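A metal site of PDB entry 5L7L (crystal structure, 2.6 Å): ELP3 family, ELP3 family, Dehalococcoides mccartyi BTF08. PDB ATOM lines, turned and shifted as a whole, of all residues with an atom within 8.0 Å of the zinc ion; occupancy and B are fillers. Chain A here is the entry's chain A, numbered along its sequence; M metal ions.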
ATOM      1  N   LEU A 228     -32.991   2.425   2.153  1.00  0.00           N
ATOM      2  CA  LEU A 228     -33.769   1.435   2.872  1.00  0.00           C
ATOM      3  C   LEU A 228     -32.840   0.513   3.640  1.00  0.00           C
ATOM      4  O   LEU A 228     -31.911  -0.072   3.077  1.00  0.00           O
ATOM      5  CB  LEU A 228     -34.624   0.598   1.914  1.00  0.00           C
ATOM      6  CG  LEU A 228     -35.933   1.186   1.402  1.00  0.00           C
ATOM      7  CD1 LEU A 228     -36.657   0.153   0.561  1.00  0.00           C
ATOM      8  CD2 LEU A 228     -36.811   1.631   2.556  1.00  0.00           C
ATOM      9  N   LEU A 230     -32.978  -2.857   5.244  1.00  0.00           N
ATOM     10  CA  LEU A 230     -33.828  -4.043   5.229  1.00  0.00           C
ATOM     11  C   LEU A 230     -33.582  -4.957   6.420  1.00  0.00           C
ATOM     12  O   LEU A 230     -32.490  -5.512   6.571  1.00  0.00           O
ATOM     13  CB  LEU A 230     -33.616  -4.823   3.942  1.00  0.00           C
ATOM     14  CG  LEU A 230     -34.142  -4.176   2.653  1.00  0.00           C
ATOM     15  CD1 LEU A 230     -33.691  -4.961   1.439  1.00  0.00           C
ATOM     16  CD2 LEU A 230     -35.652  -4.083   2.695  1.00  0.00           C
ATOM     17  N   LYS A 266     -35.243  -5.037  -4.418  1.00  0.00           N
ATOM     18  CA  LYS A 266     -34.016  -4.459  -4.956  1.00  0.00           C
ATOM     19  C   LYS A 266     -34.174  -4.141  -6.437  1.00  0.00           C
ATOM     20  O   LYS A 266     -33.494  -3.266  -6.966  1.00  0.00           O
ATOM     21  CB  LYS A 266     -32.839  -5.402  -4.755  1.00  0.00           C
ATOM     22  CG  LYS A 266     -32.383  -5.537  -3.309  1.00  0.00           C
ATOM     23  CD  LYS A 266     -31.045  -6.229  -3.231  1.00  0.00           C
ATOM     24  CE  LYS A 266     -30.487  -6.203  -1.815  1.00  0.00           C
ATOM     25  NZ  LYS A 266     -29.109  -6.751  -1.772  1.00  0.00           N
ATOM     26  N   VAL A 269     -35.806  -0.340  -7.084  1.00  0.00           N
ATOM     27  CA  VAL A 269     -35.308   0.877  -6.442  1.00  0.00           C
ATOM     28  C   VAL A 269     -34.800   1.883  -7.447  1.00  0.00           C
ATOM     29  O   VAL A 269     -34.093   1.531  -8.390  1.00  0.00           O
ATOM     30  CB  VAL A 269     -34.196   0.586  -5.418  1.00  0.00           C
ATOM     31  CG1 VAL A 269     -34.776  -0.085  -4.193  1.00  0.00           C
ATOM     32  CG2 VAL A 269     -33.084  -0.242  -6.047  1.00  0.00           C
ATOM     33  N   VAL A 273     -31.389   5.804  -4.622  1.00  0.00           N
ATOM     34  CA  VAL A 273     -31.621   5.093  -3.369  1.00  0.00           C
ATOM     35  C   VAL A 273     -30.496   4.120  -3.014  1.00  0.00           C
ATOM     36  O   VAL A 273     -29.937   3.456  -3.882  1.00  0.00           O
ATOM     37  CB  VAL A 273     -32.966   4.319  -3.423  1.00  0.00           C
ATOM     38  CG1 VAL A 273     -33.164   3.485  -2.171  1.00  0.00           C
ATOM     39  CG2 VAL A 273     -34.111   5.288  -3.593  1.00  0.00           C
ATOM     40  N   ARG A 274     -30.150   4.076  -1.731  1.00  0.00           N
ATOM     41  CA  ARG A 274     -29.184   3.113  -1.211  1.00  0.00           C
ATOM     42  C   ARG A 274     -29.920   1.966  -0.515  1.00  0.00           C
ATOM     43  O   ARG A 274     -30.874   2.186   0.223  1.00  0.00           O
ATOM     44  CB  ARG A 274     -28.219   3.797  -0.239  1.00  0.00           C
ATOM     45  CG  ARG A 274     -26.964   2.996   0.073  1.00  0.00           C
ATOM     46  CD  ARG A 274     -26.001   3.765   0.969  1.00  0.00           C
ATOM     47  N   ILE A 275     -29.490   0.726  -0.774  1.00  0.00           N
ATOM     48  CA  ILE A 275     -30.060  -0.423  -0.071  1.00  0.00           C
ATOM     49  C   ILE A 275     -29.009  -1.130   0.752  1.00  0.00           C
ATOM     50  O   ILE A 275     -27.926  -1.441   0.250  1.00  0.00           O
ATOM     51  CB  ILE A 275     -30.683  -1.459  -1.019  1.00  0.00           C
ATOM     52  CG1 ILE A 275     -31.628  -0.822  -2.028  1.00  0.00           C
ATOM     53  CG2 ILE A 275     -31.444  -2.527  -0.239  1.00  0.00           C
ATOM     54  CD1 ILE A 275     -32.071  -1.810  -3.072  1.00  0.00           C
ATOM     55  N   SER A 276     -29.340  -1.415   2.007  1.00  0.00           N
ATOM     56  CA  SER A 276     -28.444  -2.191   2.856  1.00  0.00           C
ATOM     57  C   SER A 276     -29.217  -3.284   3.579  1.00  0.00           C
ATOM     58  O   SER A 276     -30.366  -3.081   3.964  1.00  0.00           O
ATOM     59  CB  SER A 276     -27.736  -1.276   3.867  1.00  0.00           C
ATOM     60  OG  SER A 276     -28.646  -0.410   4.518  1.00  0.00           O
ATOM     61  N   ARG A 277     -28.594  -4.446   3.740  1.00  0.00           N
ATOM     62  CA  ARG A 277     -29.190  -5.551   4.469  1.00  0.00           C
ATOM     63  C   ARG A 277     -28.505  -5.701   5.833  1.00  0.00           C
ATOM     64  O   ARG A 277     -27.286  -5.602   5.937  1.00  0.00           O
ATOM     65  CB  ARG A 277     -29.069  -6.850   3.668  1.00  0.00           C
ATOM     66  CG  ARG A 277     -29.691  -8.071   4.331  1.00  0.00           C
ATOM     67  N   CYS A 310     -29.184  -5.708  -8.421  1.00  0.00           N
ATOM     68  CA  CYS A 310     -29.391  -4.518  -7.610  1.00  0.00           C
ATOM     69  C   CYS A 310     -28.711  -3.307  -8.233  1.00  0.00           C
ATOM     70  O   CYS A 310     -27.506  -3.318  -8.474  1.00  0.00           O
ATOM     71  CB  CYS A 310     -28.874  -4.733  -6.186  1.00  0.00           C
ATOM     72  SG  CYS A 310     -29.106  -3.327  -5.055  1.00  0.00           S
ATOM     73  N   ARG A 311     -29.503  -2.263  -8.506  1.00  0.00           N
ATOM     74  CA  ARG A 311     -28.972  -1.062  -9.123  1.00  0.00           C
ATOM     75  C   ARG A 311     -28.944   0.116  -8.147  1.00  0.00           C
ATOM     76  O   ARG A 311     -29.033   1.270  -8.565  1.00  0.00           O
ATOM     77  CB  ARG A 311     -29.798  -0.687 -10.367  1.00  0.00           C
ATOM     78  CG  ARG A 311     -29.722  -1.701 -11.490  1.00  0.00           C
ATOM     79  N   CYS A 312     -28.827  -0.170  -6.859  1.00  0.00           N
ATOM     80  CA  CYS A 312     -28.830   0.886  -5.856  1.00  0.00           C
ATOM     81  C   CYS A 312     -27.473   1.576  -5.789  1.00  0.00           C
ATOM     82  O   CYS A 312     -26.555   1.217  -6.528  1.00  0.00           O
ATOM     83  CB  CYS A 312     -29.209   0.328  -4.481  1.00  0.00           C
ATOM     84  SG  CYS A 312     -27.862  -0.534  -3.622  1.00  0.00           S
ATOM     85  N   ILE A 313     -27.356   2.556  -4.907  1.00  0.00           N
ATOM     86  CA  ILE A 313     -26.134   3.328  -4.743  1.00  0.00           C
ATOM     87  C   ILE A 313     -24.962   2.473  -4.267  1.00  0.00           C
ATOM     88  O   ILE A 313     -23.874   2.514  -4.836  1.00  0.00           O
ATOM     89  CB  ILE A 313     -26.334   4.482  -3.755  1.00  0.00           C
ATOM     90  CG1 ILE A 313     -27.354   5.479  -4.294  1.00  0.00           C
ATOM     91  CG2 ILE A 313     -25.014   5.181  -3.474  1.00  0.00           C
ATOM     92  CD1 ILE A 313     -27.664   6.591  -3.330  1.00  0.00           C
ATOM     93  N   ARG A 314     -25.211   1.702  -3.211  1.00  0.00           N
ATOM     94  CA  ARG A 314     -24.201   0.820  -2.610  1.00  0.00           C
ATOM     95  C   ARG A 314     -23.624  -0.168  -3.615  1.00  0.00           C
ATOM     96  O   ARG A 314     -22.489  -0.619  -3.486  1.00  0.00           O
ATOM     97  CB  ARG A 314     -24.818   0.066  -1.412  1.00  0.00           C
ATOM     98  CG  ARG A 314     -23.924  -1.003  -0.780  1.00  0.00           C
ATOM     99  CD  ARG A 314     -24.759  -2.091  -0.105  1.00  0.00           C
ATOM    100  NE  ARG A 314     -24.081  -3.393  -0.086  1.00  0.00           N
ATOM    101  CZ  ARG A 314     -24.691  -4.563   0.110  1.00  0.00           C
ATOM    102  NH1 ARG A 314     -23.992  -5.689   0.097  1.00  0.00           N
ATOM    103  NH2 ARG A 314     -26.000  -4.607   0.320  1.00  0.00           N
ATOM    104  N   CYS A 315     -24.392  -0.493  -4.645  1.00  0.00           N
ATOM    105  CA  CYS A 315     -24.001  -1.545  -5.580  1.00  0.00           C
ATOM    106  C   CYS A 315     -23.297  -1.002  -6.833  1.00  0.00           C
ATOM    107  O   CYS A 315     -22.964  -1.765  -7.734  1.00  0.00           O
ATOM    108  CB  CYS A 315     -25.220  -2.377  -5.968  1.00  0.00           C
ATOM    109  SG  CYS A 315     -26.102  -3.082  -4.535  1.00  0.00           S
ATOM    110  N   ARG A 316     -23.069   0.309  -6.871  1.00  0.00           N
ATOM    111  CA  ARG A 316     -22.325   0.928  -7.968  1.00  0.00           C
ATOM    112  C   ARG A 316     -21.092   1.677  -7.443  1.00  0.00           C
ATOM    113  O   ARG A 316     -20.630   2.637  -8.061  1.00  0.00           O
ATOM    114  CB  ARG A 316     -23.211   1.889  -8.749  1.00  0.00           C
ATOM    115  CG  ARG A 316     -24.438   1.235  -9.377  1.00  0.00           C
ATOM    116  CD  ARG A 316     -25.316   2.268 -10.077  1.00  0.00           C
ATOM    117  NE  ARG A 316     -26.213   2.943  -9.152  1.00  0.00           N
ATOM    118  CZ  ARG A 316     -26.703   4.170  -9.336  1.00  0.00           C
ATOM    119  NH1 ARG A 316     -26.357   4.860 -10.409  1.00  0.00           N
ATOM    120  NH2 ARG A 316     -27.525   4.704  -8.439  1.00  0.00           N
HETATM  121 ZN    ZN M   1     -27.922  -2.799  -3.141  1.00  0.00          ZN
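The side-chain sulfur (SG) of Cys 312 lies close to the backbone NH (N) of Ile 275 (3.5 Å). The side-chain sulfur (SG) of Cys 312 sits close to the backbone NH (N) of Arg 314 (3.5 Å). The backbone carbonyl oxygen (O) of Cys 312 lies within hydrogen-bond range of the guanidinium group (NE) of Arg 316 (3.2 Å).
Residues that only touch the zinc ion: Ile 275 (3.7 Å).
SG of Cys 315 binds the zinc ion (2.3 Å). SG of Cys 310 is bound to the zinc ion. The zinc ion is bound by SG of Cys 312, 2.3 Å away. The zinc ion has three donor atoms within binding distance.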
